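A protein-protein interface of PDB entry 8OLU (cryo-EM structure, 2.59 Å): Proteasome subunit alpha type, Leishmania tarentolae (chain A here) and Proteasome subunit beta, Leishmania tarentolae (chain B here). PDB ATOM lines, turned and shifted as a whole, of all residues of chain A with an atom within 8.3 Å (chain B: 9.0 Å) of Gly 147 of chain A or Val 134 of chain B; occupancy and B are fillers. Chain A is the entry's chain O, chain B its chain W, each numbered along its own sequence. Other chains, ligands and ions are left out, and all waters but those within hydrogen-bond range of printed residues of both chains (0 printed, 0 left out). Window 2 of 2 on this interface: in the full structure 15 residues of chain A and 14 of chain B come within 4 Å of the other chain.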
ATOM      1  N   ASP A 141       0.386 -18.946 -21.479  1.00  0.00           N
ATOM      2  CA  ASP A 141      -0.719 -19.853 -21.336  1.00  0.00           C
ATOM      3  C   ASP A 141      -0.221 -21.169 -20.773  1.00  0.00           C
ATOM      4  O   ASP A 141       0.684 -21.755 -21.340  1.00  0.00           O
ATOM      5  CB  ASP A 141      -1.290 -20.130 -22.709  1.00  0.00           C
ATOM      6  CG  ASP A 141      -2.554 -20.954 -22.602  1.00  0.00           C
ATOM      7  OD1 ASP A 141      -3.519 -20.482 -21.869  1.00  0.00           O
ATOM      8  OD2 ASP A 141      -2.564 -22.053 -23.249  1.00  0.00           O
ATOM      9  N   GLN A 142      -0.809 -21.624 -19.672  1.00  0.00           N
ATOM     10  CA  GLN A 142      -0.292 -22.780 -18.977  1.00  0.00           C
ATOM     11  C   GLN A 142      -0.848 -23.996 -19.667  1.00  0.00           C
ATOM     12  O   GLN A 142      -1.990 -23.971 -20.095  1.00  0.00           O
ATOM     13  CB  GLN A 142      -0.687 -22.668 -17.515  1.00  0.00           C
ATOM     14  CG  GLN A 142      -0.105 -23.762 -16.628  1.00  0.00           C
ATOM     15  CD  GLN A 142      -0.116 -23.277 -15.195  1.00  0.00           C
ATOM     16  OE1 GLN A 142      -1.095 -22.680 -14.732  1.00  0.00           O
ATOM     17  NE2 GLN A 142       1.006 -23.468 -14.518  1.00  0.00           N
ATOM     18  N   SER A 143      -0.005 -24.993 -19.862  1.00  0.00           N
ATOM     19  CA  SER A 143      -0.419 -26.245 -20.459  1.00  0.00           C
ATOM     20  C   SER A 143      -0.856 -27.187 -19.354  1.00  0.00           C
ATOM     21  O   SER A 143      -0.227 -27.204 -18.306  1.00  0.00           O
ATOM     22  CB  SER A 143       0.716 -26.875 -21.212  1.00  0.00           C
ATOM     23  OG  SER A 143       1.278 -27.950 -20.445  1.00  0.00           O
ATOM     24  N   ASP A 144      -1.855 -28.033 -19.623  1.00  0.00           N
ATOM     25  CA  ASP A 144      -2.341 -28.982 -18.633  1.00  0.00           C
ATOM     26  C   ASP A 144      -1.398 -30.167 -18.412  1.00  0.00           C
ATOM     27  O   ASP A 144      -1.421 -30.725 -17.317  1.00  0.00           O
ATOM     28  CB  ASP A 144      -3.675 -29.612 -19.031  1.00  0.00           C
ATOM     29  CG  ASP A 144      -4.799 -28.641 -19.341  1.00  0.00           C
ATOM     30  OD1 ASP A 144      -4.950 -27.640 -18.575  1.00  0.00           O
ATOM     31  OD2 ASP A 144      -5.548 -28.929 -20.341  1.00  0.00           O
ATOM     32  N   GLN A 145      -0.587 -30.577 -19.401  1.00  0.00           N
ATOM     33  CA  GLN A 145       0.334 -31.690 -19.192  1.00  0.00           C
ATOM     34  C   GLN A 145       1.401 -31.343 -18.140  1.00  0.00           C
ATOM     35  O   GLN A 145       1.407 -31.911 -17.051  1.00  0.00           O
ATOM     36  CB  GLN A 145       0.941 -32.137 -20.523  1.00  0.00           C
ATOM     37  CG  GLN A 145      -0.083 -32.841 -21.407  1.00  0.00           C
ATOM     38  CD  GLN A 145      -0.049 -32.338 -22.833  1.00  0.00           C
ATOM     39  OE1 GLN A 145       0.803 -32.731 -23.628  1.00  0.00           O
ATOM     40  NE2 GLN A 145      -0.986 -31.462 -23.168  1.00  0.00           N
ATOM     41  N   ASP A 146       2.285 -30.392 -18.457  1.00  0.00           N
ATOM     42  CA  ASP A 146       3.481 -30.148 -17.664  1.00  0.00           C
ATOM     43  C   ASP A 146       3.313 -28.919 -16.767  1.00  0.00           C
ATOM     44  O   ASP A 146       4.072 -28.780 -15.808  1.00  0.00           O
ATOM     45  CB  ASP A 146       4.741 -30.044 -18.554  1.00  0.00           C
ATOM     46  CG  ASP A 146       4.544 -29.499 -19.976  1.00  0.00           C
ATOM     47  OD1 ASP A 146       4.957 -30.182 -20.939  1.00  0.00           O
ATOM     48  OD2 ASP A 146       3.972 -28.391 -20.126  1.00  0.00           O
ATOM     49  N   GLY A 147       2.384 -28.001 -17.098  1.00  0.00           N
ATOM     50  CA  GLY A 147       2.229 -26.756 -16.359  1.00  0.00           C
ATOM     51  C   GLY A 147       3.158 -25.658 -16.878  1.00  0.00           C
ATOM     52  O   GLY A 147       3.192 -24.541 -16.363  1.00  0.00           O
ATOM     53  N   SER A 148       3.863 -25.966 -17.970  1.00  0.00           N
ATOM     54  CA  SER A 148       4.750 -25.010 -18.595  1.00  0.00           C
ATOM     55  C   SER A 148       3.922 -23.954 -19.314  1.00  0.00           C
ATOM     56  O   SER A 148       2.822 -24.222 -19.786  1.00  0.00           O
ATOM     57  CB  SER A 148       5.738 -25.690 -19.525  1.00  0.00           C
ATOM     58  OG  SER A 148       5.061 -26.365 -20.582  1.00  0.00           O
ATOM     59  N   LEU A 149       4.524 -22.767 -19.428  1.00  0.00           N
ATOM     60  CA  LEU A 149       3.896 -21.614 -20.018  1.00  0.00           C
ATOM     61  C   LEU A 149       4.335 -21.568 -21.467  1.00  0.00           C
ATOM     62  O   LEU A 149       5.514 -21.642 -21.768  1.00  0.00           O
ATOM     63  CB  LEU A 149       4.346 -20.370 -19.248  1.00  0.00           C
ATOM     64  CG  LEU A 149       3.792 -20.197 -17.839  1.00  0.00           C
ATOM     65  CD1 LEU A 149       3.916 -18.764 -17.322  1.00  0.00           C
ATOM     66  CD2 LEU A 149       2.336 -20.591 -17.769  1.00  0.00           C
ATOM     67  N   LYS A 150       3.351 -21.485 -22.362  1.00  0.00           N
ATOM     68  CA  LYS A 150       3.598 -21.257 -23.768  1.00  0.00           C
ATOM     69  C   LYS A 150       3.034 -19.903 -24.067  1.00  0.00           C
ATOM     70  O   LYS A 150       1.997 -19.523 -23.560  1.00  0.00           O
ATOM     71  CB  LYS A 150       2.912 -22.198 -24.752  1.00  0.00           C
ATOM     72  CG  LYS A 150       2.937 -23.683 -24.384  1.00  0.00           C
ATOM     73  CD  LYS A 150       1.988 -24.508 -25.287  1.00  0.00           C
ATOM     74  CE  LYS A 150       0.528 -24.056 -25.262  1.00  0.00           C
ATOM     75  NZ  LYS A 150       0.049 -23.681 -26.621  1.00  0.00           N
ATOM     76  N   ASN B  69     -11.630 -34.851 -13.654  1.00  0.00           N
ATOM     77  CA  ASN B  69     -10.556 -34.799 -12.696  1.00  0.00           C
ATOM     78  C   ASN B  69     -11.013 -34.175 -11.384  1.00  0.00           C
ATOM     79  O   ASN B  69     -10.203 -33.838 -10.531  1.00  0.00           O
ATOM     80  CB  ASN B  69      -9.415 -33.952 -13.261  1.00  0.00           C
ATOM     81  CG  ASN B  69      -9.811 -32.534 -13.539  1.00  0.00           C
ATOM     82  OD1 ASN B  69     -10.969 -32.344 -13.858  1.00  0.00           O
ATOM     83  ND2 ASN B  69      -8.920 -31.573 -13.371  1.00  0.00           N
ATOM     84  N   LYS B 101      -9.368 -26.585 -22.188  1.00  0.00           N
ATOM     85  CA  LYS B 101      -8.471 -27.042 -21.142  1.00  0.00           C
ATOM     86  C   LYS B 101      -9.284 -27.883 -20.175  1.00  0.00           C
ATOM     87  O   LYS B 101     -10.485 -27.986 -20.283  1.00  0.00           O
ATOM     88  CB  LYS B 101      -7.914 -25.879 -20.317  1.00  0.00           C
ATOM     89  CG  LYS B 101      -7.238 -24.745 -21.067  1.00  0.00           C
ATOM     90  CD  LYS B 101      -5.784 -25.034 -21.336  1.00  0.00           C
ATOM     91  CE  LYS B 101      -5.066 -23.864 -21.997  1.00  0.00           C
ATOM     92  NZ  LYS B 101      -3.899 -24.331 -22.805  1.00  0.00           N
ATOM     93  N   GLN B 102      -8.561 -28.527 -19.287  1.00  0.00           N
ATOM     94  CA  GLN B 102      -9.036 -29.248 -18.137  1.00  0.00           C
ATOM     95  C   GLN B 102      -9.593 -28.293 -17.094  1.00  0.00           C
ATOM     96  O   GLN B 102      -9.016 -27.248 -16.836  1.00  0.00           O
ATOM     97  CB  GLN B 102      -7.785 -29.940 -17.608  1.00  0.00           C
ATOM     98  CG  GLN B 102      -8.049 -30.948 -16.534  1.00  0.00           C
ATOM     99  CD  GLN B 102      -6.821 -31.629 -15.979  1.00  0.00           C
ATOM    100  OE1 GLN B 102      -5.848 -30.973 -15.586  1.00  0.00           O
ATOM    101  NE2 GLN B 102      -6.912 -32.948 -15.902  1.00  0.00           N
ATOM    102  N   SER B 103     -10.643 -28.705 -16.402  1.00  0.00           N
ATOM    103  CA  SER B 103     -11.224 -27.850 -15.405  1.00  0.00           C
ATOM    104  C   SER B 103     -10.305 -27.776 -14.219  1.00  0.00           C
ATOM    105  O   SER B 103      -9.725 -28.761 -13.789  1.00  0.00           O
ATOM    106  CB  SER B 103     -12.539 -28.335 -14.985  1.00  0.00           C
ATOM    107  OG  SER B 103     -13.480 -28.357 -16.054  1.00  0.00           O
ATOM    108  N   ARG B 104     -10.194 -26.586 -13.680  1.00  0.00           N
ATOM    109  CA  ARG B 104      -9.390 -26.385 -12.500  1.00  0.00           C
ATOM    110  C   ARG B 104     -10.278 -26.578 -11.266  1.00  0.00           C
ATOM    111  O   ARG B 104     -11.417 -26.127 -11.187  1.00  0.00           O
ATOM    112  CB  ARG B 104      -8.832 -24.975 -12.397  1.00  0.00           C
ATOM    113  CG  ARG B 104      -7.974 -24.480 -13.547  1.00  0.00           C
ATOM    114  CD  ARG B 104      -6.673 -25.188 -13.706  1.00  0.00           C
ATOM    115  NE  ARG B 104      -5.880 -24.564 -14.768  1.00  0.00           N
ATOM    116  CZ  ARG B 104      -4.877 -23.713 -14.562  1.00  0.00           C
ATOM    117  NH1 ARG B 104      -3.962 -23.539 -15.501  1.00  0.00           N
ATOM    118  NH2 ARG B 104      -4.795 -23.075 -13.401  1.00  0.00           N
ATOM    119  N   VAL B 105      -9.713 -27.212 -10.245  1.00  0.00           N
ATOM    120  CA  VAL B 105     -10.505 -27.436  -9.076  1.00  0.00           C
ATOM    121  C   VAL B 105     -10.902 -26.124  -8.435  1.00  0.00           C
ATOM    122  O   VAL B 105     -11.910 -26.029  -7.755  1.00  0.00           O
ATOM    123  CB  VAL B 105      -9.740 -28.292  -8.090  1.00  0.00           C
ATOM    124  CG1 VAL B 105     -10.640 -28.643  -6.920  1.00  0.00           C
ATOM    125  CG2 VAL B 105      -9.182 -29.533  -8.753  1.00  0.00           C
ATOM    126  N   LEU B 106     -10.082 -25.115  -8.622  1.00  0.00           N
ATOM    127  CA  LEU B 106     -10.399 -23.864  -7.996  1.00  0.00           C
ATOM    128  C   LEU B 106     -11.515 -23.126  -8.746  1.00  0.00           C
ATOM    129  O   LEU B 106     -12.219 -22.368  -8.098  1.00  0.00           O
ATOM    130  CB  LEU B 106      -9.103 -23.063  -7.897  1.00  0.00           C
ATOM    131  CG  LEU B 106      -9.299 -21.598  -7.491  1.00  0.00           C
ATOM    132  CD1 LEU B 106      -9.840 -21.442  -6.038  1.00  0.00           C
ATOM    133  CD2 LEU B 106      -8.012 -20.855  -7.654  1.00  0.00           C
ATOM    134  N   GLY B 131      -9.996 -32.634  -6.468  1.00  0.00           N
ATOM    135  CA  GLY B 131      -9.554 -32.974  -7.778  1.00  0.00           C
ATOM    136  C   GLY B 131      -8.067 -32.807  -7.923  1.00  0.00           C
ATOM    137  O   GLY B 131      -7.385 -32.512  -6.986  1.00  0.00           O
ATOM    138  N   VAL B 132      -7.619 -32.976  -9.134  1.00  0.00           N
ATOM    139  CA  VAL B 132      -6.232 -32.829  -9.449  1.00  0.00           C
ATOM    140  C   VAL B 132      -6.181 -32.062 -10.722  1.00  0.00           C
ATOM    141  O   VAL B 132      -6.898 -32.359 -11.635  1.00  0.00           O
ATOM    142  CB  VAL B 132      -5.559 -34.201  -9.534  1.00  0.00           C
ATOM    143  CG1 VAL B 132      -4.107 -34.109  -9.790  1.00  0.00           C
ATOM    144  CG2 VAL B 132      -5.730 -34.932  -8.213  1.00  0.00           C
ATOM    145  N   ASP B 133      -5.434 -31.008 -10.694  1.00  0.00           N
ATOM    146  CA  ASP B 133      -5.308 -30.232 -11.883  1.00  0.00           C
ATOM    147  C   ASP B 133      -3.813 -30.107 -12.096  1.00  0.00           C
ATOM    148  O   ASP B 133      -3.043 -30.953 -11.642  1.00  0.00           O
ATOM    149  CB  ASP B 133      -6.250 -29.011 -11.861  1.00  0.00           C
ATOM    150  CG  ASP B 133      -5.973 -27.896 -10.850  1.00  0.00           C
ATOM    151  OD1 ASP B 133      -4.777 -27.457 -10.801  1.00  0.00           O
ATOM    152  OD2 ASP B 133      -6.965 -27.405 -10.140  1.00  0.00           O
ATOM    153  N   VAL B 134      -3.450 -29.159 -12.935  1.00  0.00           N
ATOM    154  CA  VAL B 134      -2.082 -28.962 -13.355  1.00  0.00           C
ATOM    155  C   VAL B 134      -1.261 -28.506 -12.155  1.00  0.00           C
ATOM    156  O   VAL B 134      -0.121 -28.909 -11.986  1.00  0.00           O
ATOM    157  CB  VAL B 134      -2.072 -27.928 -14.495  1.00  0.00           C
ATOM    158  CG1 VAL B 134      -2.578 -26.539 -14.070  1.00  0.00           C
ATOM    159  CG2 VAL B 134      -0.688 -27.835 -15.069  1.00  0.00           C
ATOM    160  N   GLU B 135      -1.916 -27.751 -11.276  1.00  0.00           N
ATOM    161  CA  GLU B 135      -1.324 -27.241 -10.055  1.00  0.00           C
ATOM    162  C   GLU B 135      -1.221 -28.276  -8.924  1.00  0.00           C
ATOM    163  O   GLU B 135      -0.758 -27.926  -7.852  1.00  0.00           O
ATOM    164  CB  GLU B 135      -2.147 -26.021  -9.621  1.00  0.00           C
ATOM    165  CG  GLU B 135      -1.648 -24.771 -10.302  1.00  0.00           C
ATOM    166  CD  GLU B 135      -2.344 -23.458  -9.981  1.00  0.00           C
ATOM    167  OE1 GLU B 135      -3.248 -23.460  -9.101  1.00  0.00           O
ATOM    168  OE2 GLU B 135      -1.972 -22.431 -10.633  1.00  0.00           O
ATOM    169  N   GLY B 136      -1.738 -29.493  -9.125  1.00  0.00           N
ATOM    170  CA  GLY B 136      -1.620 -30.601  -8.183  1.00  0.00           C
ATOM    171  C   GLY B 136      -2.919 -30.925  -7.460  1.00  0.00           C
ATOM    172  O   GLY B 136      -4.006 -30.489  -7.828  1.00  0.00           O
ATOM    173  N   PRO B 137      -2.872 -31.705  -6.372  1.00  0.00           N
ATOM    174  CA  PRO B 137      -4.092 -32.109  -5.687  1.00  0.00           C
ATOM    175  C   PRO B 137      -4.724 -30.924  -4.994  1.00  0.00           C
ATOM    176  O   PRO B 137      -4.070 -30.000  -4.589  1.00  0.00           O
ATOM    177  CB  PRO B 137      -3.661 -33.113  -4.645  1.00  0.00           C
ATOM    178  CG  PRO B 137      -2.308 -33.481  -5.096  1.00  0.00           C
ATOM    179  CD  PRO B 137      -1.681 -32.280  -5.760  1.00  0.00           C
ATOM    180  N   PHE B 138      -6.028 -31.012  -4.878  1.00  0.00           N
ATOM    181  CA  PHE B 138      -6.736 -29.906  -4.346  1.00  0.00           C
ATOM    182  C   PHE B 138      -7.936 -30.414  -3.618  1.00  0.00           C
ATOM    183  O   PHE B 138      -8.884 -30.829  -4.220  1.00  0.00           O
ATOM    184  CB  PHE B 138      -7.217 -29.008  -5.454  1.00  0.00           C
ATOM    185  CG  PHE B 138      -7.772 -27.700  -4.974  1.00  0.00           C
ATOM    186  CD1 PHE B 138      -8.990 -27.634  -4.322  1.00  0.00           C
ATOM    187  CD2 PHE B 138      -7.061 -26.545  -5.162  1.00  0.00           C
ATOM    188  CE1 PHE B 138      -9.463 -26.428  -3.805  1.00  0.00           C
ATOM    189  CE2 PHE B 138      -7.565 -25.333  -4.748  1.00  0.00           C
ATOM    190  CZ  PHE B 138      -8.748 -25.278  -4.031  1.00  0.00           C
ATOM    191  N   THR B 208      -6.256 -39.206  -9.533  1.00  0.00           N
ATOM    192  CA  THR B 208      -4.881 -38.899  -9.825  1.00  0.00           C
ATOM    193  C   THR B 208      -4.958 -37.906 -10.959  1.00  0.00           C
ATOM    194  O   THR B 208      -6.065 -37.511 -11.319  1.00  0.00           O
ATOM    195  CB  THR B 208      -4.079 -40.183 -10.045  1.00  0.00           C
ATOM    196  OG1 THR B 208      -4.455 -40.852 -11.247  1.00  0.00           O
ATOM    197  CG2 THR B 208      -4.236 -41.157  -8.893  1.00  0.00           C
ATOM    198  N   LYS B 209      -3.778 -37.424 -11.355  1.00  0.00           N
ATOM    199  CA  LYS B 209      -3.593 -36.550 -12.498  1.00  0.00           C
ATOM    200  C   LYS B 209      -4.290 -37.161 -13.722  1.00  0.00           C
ATOM    201  O   LYS B 209      -5.063 -36.495 -14.416  1.00  0.00           O
ATOM    202  CB  LYS B 209      -2.076 -36.386 -12.632  1.00  0.00           C
ATOM    203  CG  LYS B 209      -1.582 -35.638 -13.857  1.00  0.00           C
ATOM    204  CD  LYS B 209      -0.229 -34.930 -13.658  1.00  0.00           C
ATOM    205  CE  LYS B 209       0.064 -33.871 -14.714  1.00  0.00           C
ATOM    206  NZ  LYS B 209      -1.050 -32.904 -14.908  1.00  0.00           N
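NZ of Lys 101 of chain B lies within salt-bridge range of OD2 of Asp 141 of chain A. The backbone carbonyl oxygen (O) of Gln 142 of chain A lies within hydrogen-bond range of the side-chain amino group (NZ) of Lys 101 of chain B (3.3 Å). OE1 of Gln 142 of chain A lies within hydrogen-bond range of NH1 of Arg 104 of chain B, at 3.1 Å. OD2 of Asp 144 of chain A lies within hydrogen-bond range of N of Gln 102 of chain B (3.2 Å). NZ of Lys 209 of chain B lies within hydrogen-bond range of O of Asp 144 of chain A, 3.3 Å away. O of Gln 145 of chain A lies close to NZ of Lys 209 of chain B (3.4 Å).
N of Asp 141 of chain A lies within hydrogen-bond range of O of Lys 150 of chain A, 2.7 Å away. NE2 of Gln 142 of chain A lies within hydrogen-bond range of O of Gly 147 of chain A, 3.1 Å away. N of Gln 145 of chain A is in hydrogen-bond range of OG of Ser 143 of chain A (3.4 Å). The side-chain hydroxyl (OG) of Ser 143 of chain A lies within hydrogen-bond range of the side-chain carboxylate (OD2) of Asp 146 of chain A, at 2.7 Å. The backbone NH of Ser 143 of chain A sits at hydrogen-bond distance from the backbone carbonyl oxygen of Ser 148 of chain A (2.9 Å).
Ser 143 of chain A touches Val 134 of chain B (O to CG2, 3.3 Å). CA of Lys 101 of chain B touches OD2 of Asp 144 of chain A (3.6 Å). Val 134 of chain B touches Asp 144 of chain A (CG2 to O, 3.7 Å). Val 134 of chain B touches Gly 147 of chain A (CG2 to CA, 3.4 Å).
Of the printed residues of chain B, Asp 141 of chain A touches Lys 101. Of the printed residues of chain B, Asp 144 of chain A touches Lys 101, Gln 102, Val 134 and Lys 209. Printed residues of chain B within 4 Å of Gln 145 of chain A: Lys 209 (3.3 Å). Of chain B, only Val 134 comes within 4 Å of Gly 147 of chain A. Of the printed residues of chain A, Gln 102 of chain B touches Asp 144. Of the printed residues of chain A, Arg 104 of chain B touches Gln 142 (3.1 Å). Val 105 of chain B touches none of the printed residues of chain A. Val 134 of chain B touches just these residues of chain A: Ser 143 (3.3 Å), Asp 144 (3.7 Å) and Gly 147 (3.4 Å). The nearest residue of chain A that does not touch Val 134 of chain B is Gln 142 of chain A (4.2 Å). The nearest printed residue of chain A that does not touch Lys 101 of chain B is Ser 143 of chain A (4.6 Å).
Of the 17 printed residues of chain B, 5 touch a printed residue of chain A. Of the 10 printed residues of chain A, 6 touch a printed residue of chain B. Printed residues of chain A that touch a printed residue of chain B: Asp 141, Gln 142, Ser 143, Asp 144, Gln 145 and Gly 147.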
